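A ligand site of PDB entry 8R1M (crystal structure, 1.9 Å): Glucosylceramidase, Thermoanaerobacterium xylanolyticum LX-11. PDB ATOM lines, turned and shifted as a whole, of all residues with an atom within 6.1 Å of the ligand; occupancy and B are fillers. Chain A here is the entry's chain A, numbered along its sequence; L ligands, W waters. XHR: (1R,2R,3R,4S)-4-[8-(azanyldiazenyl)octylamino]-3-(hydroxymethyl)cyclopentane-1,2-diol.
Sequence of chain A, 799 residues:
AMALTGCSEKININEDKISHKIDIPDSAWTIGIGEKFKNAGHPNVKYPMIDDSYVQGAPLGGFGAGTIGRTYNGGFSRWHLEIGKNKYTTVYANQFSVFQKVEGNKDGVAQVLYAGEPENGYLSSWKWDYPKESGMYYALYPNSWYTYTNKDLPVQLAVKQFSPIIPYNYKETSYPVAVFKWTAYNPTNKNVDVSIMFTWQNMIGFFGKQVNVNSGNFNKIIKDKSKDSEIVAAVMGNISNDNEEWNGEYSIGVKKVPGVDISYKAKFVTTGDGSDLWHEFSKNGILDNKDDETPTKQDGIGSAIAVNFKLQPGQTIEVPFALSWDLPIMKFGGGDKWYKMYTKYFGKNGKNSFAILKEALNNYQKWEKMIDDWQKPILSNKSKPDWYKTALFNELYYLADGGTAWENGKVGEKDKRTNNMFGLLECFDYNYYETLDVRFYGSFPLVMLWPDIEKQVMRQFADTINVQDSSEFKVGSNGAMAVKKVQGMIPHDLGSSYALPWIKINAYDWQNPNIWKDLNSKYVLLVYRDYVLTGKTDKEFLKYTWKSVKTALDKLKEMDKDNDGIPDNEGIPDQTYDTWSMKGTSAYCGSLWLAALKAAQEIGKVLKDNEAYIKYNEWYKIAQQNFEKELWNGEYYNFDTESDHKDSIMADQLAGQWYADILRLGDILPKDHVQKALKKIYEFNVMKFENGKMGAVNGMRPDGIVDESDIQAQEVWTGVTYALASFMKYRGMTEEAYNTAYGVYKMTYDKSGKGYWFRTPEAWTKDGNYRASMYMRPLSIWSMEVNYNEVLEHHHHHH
The side-chain carboxylate (OE2) of Glu 762 lies within hydrogen-bond range of an oxygen (O3) of the ligand (2.8 Å).
N4 of the ligand is in salt-bridge range of OD2 of Asp 578 (2.8 Å).
An oxygen (O2) of the ligand sits at hydrogen-bond distance from the backbone carbonyl oxygen of Thr 576, at 2.6 Å.
The side-chain carboxylate of Glu 426 is covalently linked to a carbon (C10) of the ligand, at 1.5 Å.
The guanidinium group (NH1) of Arg 771 sits at hydrogen-bond distance from an oxygen (O3) of the ligand (2.8 Å).
The guanidinium group (NH2) of Arg 777 sits at hydrogen-bond distance from an oxygen (O2) of the ligand (2.9 Å).
O1 of the ligand sits at hydrogen-bond distance from NE2 of His 492 (2.7 Å).
OG1 of Thr 576 lies within hydrogen-bond range of O2 of the ligand, at 2.7 Å.
The side-chain carboxylate of Asp 437 lies within hydrogen-bond range of an oxygen (O1) of the ligand, 2.7 Å away.
The side-chain carboxylate of Glu 715 sits at hydrogen-bond distance from the indole nitrogen of Trp 717, at 3.0 Å.
The guanidinium group (NH1) of Arg 771 sits at hydrogen-bond distance from the side-chain hydroxyl (OH) of Tyr 430, at 3.0 Å.
The backbone NH (N) of Glu 762 lies within hydrogen-bond range of the backbone carbonyl oxygen (O) of Ala 772 (3.0 Å).
OD1 of Asp 578 sits at hydrogen-bond distance from NE2 of Gln 712, 3.1 Å away.
O of Asp 578 sits at hydrogen-bond distance from NE1 of Trp 510 (3.2 Å).
OH of Tyr 508 is in hydrogen-bond range of OD2 of Asp 578.
The side-chain carboxylate (OE2) of Glu 426 sits at hydrogen-bond distance from the side-chain hydroxyl (OG1) of Thr 435 (3.2 Å).
OD2 of Asp 437 sits at hydrogen-bond distance from OG1 of Thr 576 (2.6 Å).
Tyr 47 touches the ligand.
Tyr 430 touches the ligand.
Thr 435 touches the ligand (CG2 to O1, 3.4 Å).
Val 438 touches the ligand.
CE1 of Tyr 508 touches C8 of the ligand, at 3.9 Å.
Trp 510 touches the ligand (CB to C5, 3.8 Å).
Trp 516 touches the ligand (CH2 to O1, 3.99 Å).
Trp 717 touches the ligand (CH2 to C14, 3.7 Å).
OH of Tyr 775 touches C13 of the ligand, 3.3 Å away.
Water W1 lies within hydrogen-bond range of OD1 of Asp 578 (2.6 Å), N4 of the ligand (2.8 Å), NH1 of Arg 771 (3.4 Å) and NE2 of Gln 712 (3.5 Å).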
ATOM      1  N   TYR A  47     -10.461   2.840   5.471  1.00  0.00           N
ATOM      2  CA  TYR A  47     -10.078   1.449   5.258  1.00  0.00           C
ATOM      3  C   TYR A  47      -9.120   1.373   4.072  1.00  0.00           C
ATOM      4  O   TYR A  47      -9.080   2.282   3.260  1.00  0.00           O
ATOM      5  CB  TYR A  47     -11.336   0.585   5.093  1.00  0.00           C
ATOM      6  CG  TYR A  47     -12.342   1.023   4.022  1.00  0.00           C
ATOM      7  CD1 TYR A  47     -13.393   1.883   4.305  1.00  0.00           C
ATOM      8  CD2 TYR A  47     -12.286   0.482   2.738  1.00  0.00           C
ATOM      9  CE1 TYR A  47     -14.333   2.237   3.337  1.00  0.00           C
ATOM     10  CE2 TYR A  47     -13.213   0.818   1.758  1.00  0.00           C
ATOM     11  CZ  TYR A  47     -14.237   1.700   2.055  1.00  0.00           C
ATOM     12  OH  TYR A  47     -15.109   2.003   1.031  1.00  0.00           O
ATOM     13  N   GLU A 426     -17.922  -4.975 -10.348  1.00  0.00           N
ATOM     14  CA  GLU A 426     -18.197  -3.680  -9.764  1.00  0.00           C
ATOM     15  C   GLU A 426     -16.908  -2.875  -9.723  1.00  0.00           C
ATOM     16  O   GLU A 426     -16.901  -1.767 -10.236  1.00  0.00           O
ATOM     17  CB  GLU A 426     -18.863  -3.843  -8.395  1.00  0.00           C
ATOM     18  CG  GLU A 426     -19.125  -2.538  -7.641  1.00  0.00           C
ATOM     19  CD  GLU A 426     -19.960  -2.604  -6.359  1.00  0.00           C
ATOM     20  OE1 GLU A 426     -20.173  -1.520  -5.726  1.00  0.00           O
ATOM     21  OE2 GLU A 426     -20.423  -3.717  -6.041  1.00  0.00           O
ATOM     22  N   TYR A 430     -14.336  -3.682  -4.383  1.00  0.00           N
ATOM     23  CA  TYR A 430     -15.630  -4.269  -4.099  1.00  0.00           C
ATOM     24  C   TYR A 430     -15.833  -5.378  -5.120  1.00  0.00           C
ATOM     25  O   TYR A 430     -16.434  -5.155  -6.163  1.00  0.00           O
ATOM     26  CB  TYR A 430     -16.749  -3.216  -4.204  1.00  0.00           C
ATOM     27  CG  TYR A 430     -16.528  -1.909  -3.460  1.00  0.00           C
ATOM     28  CD1 TYR A 430     -15.894  -1.861  -2.224  1.00  0.00           C
ATOM     29  CD2 TYR A 430     -16.973  -0.712  -3.990  1.00  0.00           C
ATOM     30  CE1 TYR A 430     -15.708  -0.667  -1.546  1.00  0.00           C
ATOM     31  CE2 TYR A 430     -16.798   0.493  -3.331  1.00  0.00           C
ATOM     32  CZ  TYR A 430     -16.140   0.520  -2.115  1.00  0.00           C
ATOM     33  OH  TYR A 430     -15.993   1.718  -1.501  1.00  0.00           O
ATOM     34  N   TYR A 432     -17.234  -7.850  -6.718  1.00  0.00           N
ATOM     35  CA  TYR A 432     -18.474  -8.571  -6.978  1.00  0.00           C
ATOM     36  C   TYR A 432     -18.809  -8.511  -8.469  1.00  0.00           C
ATOM     37  O   TYR A 432     -18.746  -7.429  -9.054  1.00  0.00           O
ATOM     38  CB  TYR A 432     -19.575  -7.882  -6.191  1.00  0.00           C
ATOM     39  CG  TYR A 432     -19.219  -7.666  -4.732  1.00  0.00           C
ATOM     40  CD1 TYR A 432     -18.910  -8.735  -3.908  1.00  0.00           C
ATOM     41  CD2 TYR A 432     -19.158  -6.384  -4.200  1.00  0.00           C
ATOM     42  CE1 TYR A 432     -18.596  -8.552  -2.574  1.00  0.00           C
ATOM     43  CE2 TYR A 432     -18.836  -6.186  -2.863  1.00  0.00           C
ATOM     44  CZ  TYR A 432     -18.534  -7.274  -2.050  1.00  0.00           C
ATOM     45  OH  TYR A 432     -18.181  -7.080  -0.743  1.00  0.00           O
ATOM     46  N   THR A 435     -22.743  -6.551 -10.315  1.00  0.00           N
ATOM     47  CA  THR A 435     -23.603  -5.813  -9.404  1.00  0.00           C
ATOM     48  C   THR A 435     -24.709  -5.111 -10.175  1.00  0.00           C
ATOM     49  O   THR A 435     -24.482  -4.114 -10.868  1.00  0.00           O
ATOM     50  CB  THR A 435     -22.723  -4.819  -8.654  1.00  0.00           C
ATOM     51  OG1 THR A 435     -21.746  -5.722  -8.139  1.00  0.00           O
ATOM     52  CG2 THR A 435     -23.511  -4.037  -7.622  1.00  0.00           C
ATOM     53  N   ASP A 437     -27.463  -3.296  -9.450  1.00  0.00           N
ATOM     54  CA  ASP A 437     -27.758  -1.918  -9.116  1.00  0.00           C
ATOM     55  C   ASP A 437     -26.763  -0.954  -9.781  1.00  0.00           C
ATOM     56  O   ASP A 437     -27.087   0.217  -9.945  1.00  0.00           O
ATOM     57  CB  ASP A 437     -27.727  -1.685  -7.618  1.00  0.00           C
ATOM     58  CG  ASP A 437     -26.450  -2.086  -6.915  1.00  0.00           C
ATOM     59  OD1 ASP A 437     -26.093  -3.262  -7.059  1.00  0.00           O
ATOM     60  OD2 ASP A 437     -25.822  -1.257  -6.209  1.00  0.00           O
ATOM     61  N   VAL A 438     -25.568  -1.455 -10.111  1.00  0.00           N
ATOM     62  CA  VAL A 438     -24.531  -0.693 -10.769  1.00  0.00           C
ATOM     63  C   VAL A 438     -24.594  -0.895 -12.288  1.00  0.00           C
ATOM     64  O   VAL A 438     -24.452   0.070 -13.040  1.00  0.00           O
ATOM     65  CB  VAL A 438     -23.131  -1.049 -10.243  1.00  0.00           C
ATOM     66  CG1 VAL A 438     -22.031  -0.218 -10.912  1.00  0.00           C
ATOM     67  CG2 VAL A 438     -23.008  -0.935  -8.724  1.00  0.00           C
ATOM     68  N   HIS A 492     -27.943  -9.055  -5.625  1.00  0.00           N
ATOM     69  CA  HIS A 492     -27.056  -7.920  -5.774  1.00  0.00           C
ATOM     70  C   HIS A 492     -25.995  -8.246  -6.826  1.00  0.00           C
ATOM     71  O   HIS A 492     -25.659  -7.380  -7.617  1.00  0.00           O
ATOM     72  CB  HIS A 492     -26.396  -7.586  -4.435  1.00  0.00           C
ATOM     73  CG  HIS A 492     -25.342  -6.543  -4.489  1.00  0.00           C
ATOM     74  ND1 HIS A 492     -24.013  -6.840  -4.692  1.00  0.00           N
ATOM     75  CD2 HIS A 492     -25.403  -5.220  -4.320  1.00  0.00           C
ATOM     76  CE1 HIS A 492     -23.311  -5.718  -4.699  1.00  0.00           C
ATOM     77  NE2 HIS A 492     -24.134  -4.724  -4.460  1.00  0.00           N
ATOM     78  N   TYR A 508     -21.831  -9.979  -1.746  1.00  0.00           N
ATOM     79  CA  TYR A 508     -21.925  -8.723  -1.039  1.00  0.00           C
ATOM     80  C   TYR A 508     -22.726  -8.911   0.249  1.00  0.00           C
ATOM     81  O   TYR A 508     -23.820  -9.473   0.213  1.00  0.00           O
ATOM     82  CB  TYR A 508     -22.632  -7.751  -1.987  1.00  0.00           C
ATOM     83  CG  TYR A 508     -23.054  -6.400  -1.405  1.00  0.00           C
ATOM     84  CD1 TYR A 508     -22.189  -5.307  -1.367  1.00  0.00           C
ATOM     85  CD2 TYR A 508     -24.341  -6.208  -0.914  1.00  0.00           C
ATOM     86  CE1 TYR A 508     -22.584  -4.077  -0.874  1.00  0.00           C
ATOM     87  CE2 TYR A 508     -24.746  -4.986  -0.394  1.00  0.00           C
ATOM     88  CZ  TYR A 508     -23.868  -3.916  -0.376  1.00  0.00           C
ATOM     89  OH  TYR A 508     -24.302  -2.714   0.153  1.00  0.00           O
ATOM     90  N   TRP A 510     -22.607  -6.003   2.823  1.00  0.00           N
ATOM     91  CA  TRP A 510     -22.569  -4.778   3.596  1.00  0.00           C
ATOM     92  C   TRP A 510     -23.986  -4.385   4.013  1.00  0.00           C
ATOM     93  O   TRP A 510     -24.209  -3.924   5.129  1.00  0.00           O
ATOM     94  CB  TRP A 510     -21.852  -3.637   2.857  1.00  0.00           C
ATOM     95  CG  TRP A 510     -22.043  -2.309   3.522  1.00  0.00           C
ATOM     96  CD1 TRP A 510     -22.892  -1.322   3.110  1.00  0.00           C
ATOM     97  CD2 TRP A 510     -21.455  -1.842   4.763  1.00  0.00           C
ATOM     98  NE1 TRP A 510     -22.858  -0.278   3.990  1.00  0.00           N
ATOM     99  CE2 TRP A 510     -21.999  -0.560   5.013  1.00  0.00           C
ATOM    100  CE3 TRP A 510     -20.524  -2.372   5.671  1.00  0.00           C
ATOM    101  CZ2 TRP A 510     -21.649   0.189   6.133  1.00  0.00           C
ATOM    102  CZ3 TRP A 510     -20.173  -1.629   6.784  1.00  0.00           C
ATOM    103  CH2 TRP A 510     -20.754  -0.370   7.020  1.00  0.00           C
ATOM    104  N   TRP A 516     -33.607  -4.849  -0.768  1.00  0.00           N
ATOM    105  CA  TRP A 516     -33.397  -3.656  -1.578  1.00  0.00           C
ATOM    106  C   TRP A 516     -34.628  -3.355  -2.416  1.00  0.00           C
ATOM    107  O   TRP A 516     -35.326  -4.271  -2.867  1.00  0.00           O
ATOM    108  CB  TRP A 516     -32.155  -3.756  -2.476  1.00  0.00           C
ATOM    109  CG  TRP A 516     -30.899  -3.442  -1.707  1.00  0.00           C
ATOM    110  CD1 TRP A 516     -30.758  -3.438  -0.355  1.00  0.00           C
ATOM    111  CD2 TRP A 516     -29.613  -3.064  -2.242  1.00  0.00           C
ATOM    112  NE1 TRP A 516     -29.479  -3.103  -0.003  1.00  0.00           N
ATOM    113  CE2 TRP A 516     -28.758  -2.867  -1.142  1.00  0.00           C
ATOM    114  CE3 TRP A 516     -29.115  -2.859  -3.536  1.00  0.00           C
ATOM    115  CZ2 TRP A 516     -27.416  -2.485  -1.289  1.00  0.00           C
ATOM    116  CZ3 TRP A 516     -27.803  -2.476  -3.676  1.00  0.00           C
ATOM    117  CH2 TRP A 516     -26.953  -2.333  -2.567  1.00  0.00           C
ATOM    118  N   GLN A 575     -30.782   0.329  -1.145  1.00  0.00           N
ATOM    119  CA  GLN A 575     -30.651   0.529  -2.590  1.00  0.00           C
ATOM    120  C   GLN A 575     -29.192   0.899  -2.870  1.00  0.00           C
ATOM    121  O   GLN A 575     -28.419   0.972  -1.925  1.00  0.00           O
ATOM    122  CB  GLN A 575     -31.726   1.502  -3.109  1.00  0.00           C
ATOM    123  CG  GLN A 575     -32.050   2.673  -2.178  1.00  0.00           C
ATOM    124  CD  GLN A 575     -30.836   3.507  -1.824  1.00  0.00           C
ATOM    125  OE1 GLN A 575     -30.077   3.938  -2.700  1.00  0.00           O
ATOM    126  NE2 GLN A 575     -30.637   3.741  -0.544  1.00  0.00           N
ATOM    127  N   THR A 576     -28.854   1.174  -4.140  1.00  0.00           N
ATOM    128  CA  THR A 576     -27.470   1.288  -4.603  1.00  0.00           C
ATOM    129  C   THR A 576     -26.698   2.326  -3.784  1.00  0.00           C
ATOM    130  O   THR A 576     -25.474   2.228  -3.661  1.00  0.00           O
ATOM    131  CB  THR A 576     -27.442   1.621  -6.101  1.00  0.00           C
ATOM    132  OG1 THR A 576     -26.152   1.330  -6.661  1.00  0.00           O
ATOM    133  CG2 THR A 576     -27.781   3.060  -6.401  1.00  0.00           C
ATOM    134  N   TYR A 577     -27.383   3.334  -3.248  1.00  0.00           N
ATOM    135  CA  TYR A 577     -26.727   4.317  -2.386  1.00  0.00           C
ATOM    136  C   TYR A 577     -26.659   3.690  -0.984  1.00  0.00           C
ATOM    137  O   TYR A 577     -27.443   4.024  -0.095  1.00  0.00           O
ATOM    138  CB  TYR A 577     -27.421   5.685  -2.401  1.00  0.00           C
ATOM    139  CG  TYR A 577     -27.439   6.385  -3.747  1.00  0.00           C
ATOM    140  CD1 TYR A 577     -28.456   6.138  -4.672  1.00  0.00           C
ATOM    141  CD2 TYR A 577     -26.427   7.277  -4.124  1.00  0.00           C
ATOM    142  CE1 TYR A 577     -28.458   6.749  -5.918  1.00  0.00           C
ATOM    143  CE2 TYR A 577     -26.429   7.888  -5.370  1.00  0.00           C
ATOM    144  CZ  TYR A 577     -27.445   7.626  -6.262  1.00  0.00           C
ATOM    145  OH  TYR A 577     -27.475   8.224  -7.504  1.00  0.00           O
ATOM    146  N   ASP A 578     -25.708   2.776  -0.815  1.00  0.00           N
ATOM    147  CA  ASP A 578     -25.776   1.766   0.240  1.00  0.00           C
ATOM    148  C   ASP A 578     -25.237   2.276   1.579  1.00  0.00           C
ATOM    149  O   ASP A 578     -25.059   1.465   2.483  1.00  0.00           O
ATOM    150  CB  ASP A 578     -25.132   0.465  -0.233  1.00  0.00           C
ATOM    151  CG  ASP A 578     -23.651   0.548  -0.528  1.00  0.00           C
ATOM    152  OD1 ASP A 578     -23.104   1.678  -0.439  1.00  0.00           O
ATOM    153  OD2 ASP A 578     -23.059  -0.509  -0.858  1.00  0.00           O
ATOM    154  N   GLN A 712     -22.307   9.739   1.077  1.00  0.00           N
ATOM    155  CA  GLN A 712     -22.650   9.570  -0.327  1.00  0.00           C
ATOM    156  C   GLN A 712     -23.406  10.771  -0.902  1.00  0.00           C
ATOM    157  O   GLN A 712     -23.302  11.044  -2.101  1.00  0.00           O
ATOM    158  CB  GLN A 712     -23.426   8.283  -0.544  1.00  0.00           C
ATOM    159  CG  GLN A 712     -22.588   7.059  -0.215  1.00  0.00           C
ATOM    160  CD  GLN A 712     -23.344   5.754  -0.408  1.00  0.00           C
ATOM    161  OE1 GLN A 712     -24.584   5.695  -0.441  1.00  0.00           O
ATOM    162  NE2 GLN A 712     -22.559   4.706  -0.538  1.00  0.00           N
ATOM    163  N   GLU A 715     -20.848  13.113  -2.210  1.00  0.00           N
ATOM    164  CA  GLU A 715     -20.009  12.613  -3.287  1.00  0.00           C
ATOM    165  C   GLU A 715     -20.653  12.958  -4.627  1.00  0.00           C
ATOM    166  O   GLU A 715     -21.886  12.967  -4.781  1.00  0.00           O
ATOM    167  CB  GLU A 715     -19.801  11.090  -3.265  1.00  0.00           C
ATOM    168  CG  GLU A 715     -18.902  10.595  -2.136  1.00  0.00           C
ATOM    169  CD  GLU A 715     -18.759   9.080  -2.032  1.00  0.00           C
ATOM    170  OE1 GLU A 715     -19.780   8.373  -2.243  1.00  0.00           O
ATOM    171  OE2 GLU A 715     -17.633   8.619  -1.681  1.00  0.00           O
ATOM    172  N   TRP A 717     -21.008  11.020  -8.066  1.00  0.00           N
ATOM    173  CA  TRP A 717     -20.841   9.696  -8.643  1.00  0.00           C
ATOM    174  C   TRP A 717     -20.707   9.795 -10.156  1.00  0.00           C
ATOM    175  O   TRP A 717     -21.644  10.208 -10.832  1.00  0.00           O
ATOM    176  CB  TRP A 717     -21.987   8.739  -8.276  1.00  0.00           C
ATOM    177  CG  TRP A 717     -21.922   8.233  -6.865  1.00  0.00           C
ATOM    178  CD1 TRP A 717     -21.204   8.771  -5.839  1.00  0.00           C
ATOM    179  CD2 TRP A 717     -22.643   7.105  -6.319  1.00  0.00           C
ATOM    180  NE1 TRP A 717     -21.395   8.033  -4.700  1.00  0.00           N
ATOM    181  CE2 TRP A 717     -22.281   7.021  -4.951  1.00  0.00           C
ATOM    182  CE3 TRP A 717     -23.527   6.163  -6.844  1.00  0.00           C
ATOM    183  CZ2 TRP A 717     -22.775   6.024  -4.122  1.00  0.00           C
ATOM    184  CZ3 TRP A 717     -24.024   5.194  -6.008  1.00  0.00           C
ATOM    185  CH2 TRP A 717     -23.654   5.131  -4.664  1.00  0.00           C
ATOM    186  N   GLU A 762     -15.686   5.413  -8.671  1.00  0.00           N
ATOM    187  CA  GLU A 762     -17.096   5.586  -8.369  1.00  0.00           C
ATOM    188  C   GLU A 762     -17.349   7.068  -8.102  1.00  0.00           C
ATOM    189  O   GLU A 762     -18.269   7.652  -8.669  1.00  0.00           O
ATOM    190  CB  GLU A 762     -17.499   4.737  -7.151  1.00  0.00           C
ATOM    191  CG  GLU A 762     -18.866   5.064  -6.539  1.00  0.00           C
ATOM    192  CD  GLU A 762     -20.061   4.426  -7.193  1.00  0.00           C
ATOM    193  OE1 GLU A 762     -20.459   4.679  -8.373  1.00  0.00           O
ATOM    194  OE2 GLU A 762     -20.599   3.585  -6.449  1.00  0.00           O
ATOM    195  N   ARG A 771     -13.142   7.592  -4.139  1.00  0.00           N
ATOM    196  CA  ARG A 771     -13.492   6.296  -3.597  1.00  0.00           C
ATOM    197  C   ARG A 771     -13.726   5.327  -4.751  1.00  0.00           C
ATOM    198  O   ARG A 771     -14.452   5.656  -5.695  1.00  0.00           O
ATOM    199  CB  ARG A 771     -14.774   6.423  -2.765  1.00  0.00           C
ATOM    200  CG  ARG A 771     -15.079   5.118  -2.050  1.00  0.00           C
ATOM    201  CD  ARG A 771     -16.182   5.276  -0.997  1.00  0.00           C
ATOM    202  NE  ARG A 771     -17.463   5.744  -1.530  1.00  0.00           N
ATOM    203  CZ  ARG A 771     -18.341   4.967  -2.152  1.00  0.00           C
ATOM    204  NH1 ARG A 771     -18.104   3.676  -2.252  1.00  0.00           N
ATOM    205  NH2 ARG A 771     -19.447   5.486  -2.663  1.00  0.00           N
ATOM    206  N   ALA A 772     -13.057   4.169  -4.676  1.00  0.00           N
ATOM    207  CA  ALA A 772     -13.221   3.033  -5.573  1.00  0.00           C
ATOM    208  C   ALA A 772     -12.770   3.343  -7.015  1.00  0.00           C
ATOM    209  O   ALA A 772     -13.601   3.416  -7.923  1.00  0.00           O
ATOM    210  CB  ALA A 772     -14.649   2.546  -5.512  1.00  0.00           C
ATOM    211  N   TYR A 775     -13.840   1.496 -11.838  1.00  0.00           N
ATOM    212  CA  TYR A 775     -15.212   1.281 -11.407  1.00  0.00           C
ATOM    213  C   TYR A 775     -16.143   1.086 -12.611  1.00  0.00           C
ATOM    214  O   TYR A 775     -15.975   1.727 -13.635  1.00  0.00           O
ATOM    215  CB  TYR A 775     -15.626   2.477 -10.558  1.00  0.00           C
ATOM    216  CG  TYR A 775     -16.744   2.076  -9.619  1.00  0.00           C
ATOM    217  CD1 TYR A 775     -16.466   1.363  -8.448  1.00  0.00           C
ATOM    218  CD2 TYR A 775     -18.062   2.354  -9.917  1.00  0.00           C
ATOM    219  CE1 TYR A 775     -17.473   0.915  -7.622  1.00  0.00           C
ATOM    220  CE2 TYR A 775     -19.093   1.939  -9.089  1.00  0.00           C
ATOM    221  CZ  TYR A 775     -18.793   1.214  -7.944  1.00  0.00           C
ATOM    222  OH  TYR A 775     -19.815   0.816  -7.149  1.00  0.00           O
ATOM    223  N   ARG A 777     -19.471   1.803 -12.951  1.00  0.00           N
ATOM    224  CA  ARG A 777     -20.611   2.708 -13.146  1.00  0.00           C
ATOM    225  C   ARG A 777     -20.383   3.745 -14.259  1.00  0.00           C
ATOM    226  O   ARG A 777     -21.308   3.985 -15.030  1.00  0.00           O
ATOM    227  CB  ARG A 777     -21.078   3.416 -11.874  1.00  0.00           C
ATOM    228  CG  ARG A 777     -22.597   3.583 -11.859  1.00  0.00           C
ATOM    229  CD  ARG A 777     -23.032   4.386 -10.629  1.00  0.00           C
ATOM    230  NE  ARG A 777     -22.686   3.748  -9.343  1.00  0.00           N
ATOM    231  CZ  ARG A 777     -23.493   2.976  -8.620  1.00  0.00           C
ATOM    232  NH1 ARG A 777     -24.722   2.660  -9.025  1.00  0.00           N
ATOM    233  NH2 ARG A 777     -23.065   2.541  -7.458  1.00  0.00           N
HETATM  234  C4  XHR L   1     -17.142  -1.663   2.158  1.00  0.00           C
HETATM  235  C14 XHR L   1     -21.587   2.203  -3.613  1.00  0.00           C
HETATM  236  C5  XHR L   1     -18.389  -2.466   1.783  1.00  0.00           C
HETATM  237  C6  XHR L   1     -18.767  -2.568   0.301  1.00  0.00           C
HETATM  238  C11 XHR L   1     -22.610  -1.174  -5.082  1.00  0.00           C
HETATM  239  C7  XHR L   1     -19.640  -1.415  -0.222  1.00  0.00           C
HETATM  240  C8  XHR L   1     -19.852  -1.452  -1.736  1.00  0.00           C
HETATM  241  C9  XHR L   1     -20.699  -0.313  -3.788  1.00  0.00           C
HETATM  242  C10 XHR L   1     -21.160  -1.505  -4.658  1.00  0.00           C
HETATM  243  C12 XHR L   1     -22.944   0.169  -4.428  1.00  0.00           C
HETATM  244  C13 XHR L   1     -21.574   0.860  -4.335  1.00  0.00           C
HETATM  245  C3  XHR L   1     -16.844  -1.573   3.651  1.00  0.00           C
HETATM  246  N4  XHR L   1     -20.676  -0.370  -2.306  1.00  0.00           N
HETATM  247  O1  XHR L   1     -23.666  -2.094  -4.821  1.00  0.00           O
HETATM  248  O2  XHR L   1     -23.857   0.947  -5.200  1.00  0.00           O
HETATM  249  O3  XHR L   1     -20.363   2.922  -3.726  1.00  0.00           O
HETATM  250  C2  XHR L   1     -16.839  -0.159   4.216  1.00  0.00           C
HETATM  251  O   HOH W   1     -20.540   1.866  -0.640  1.00  0.00           O
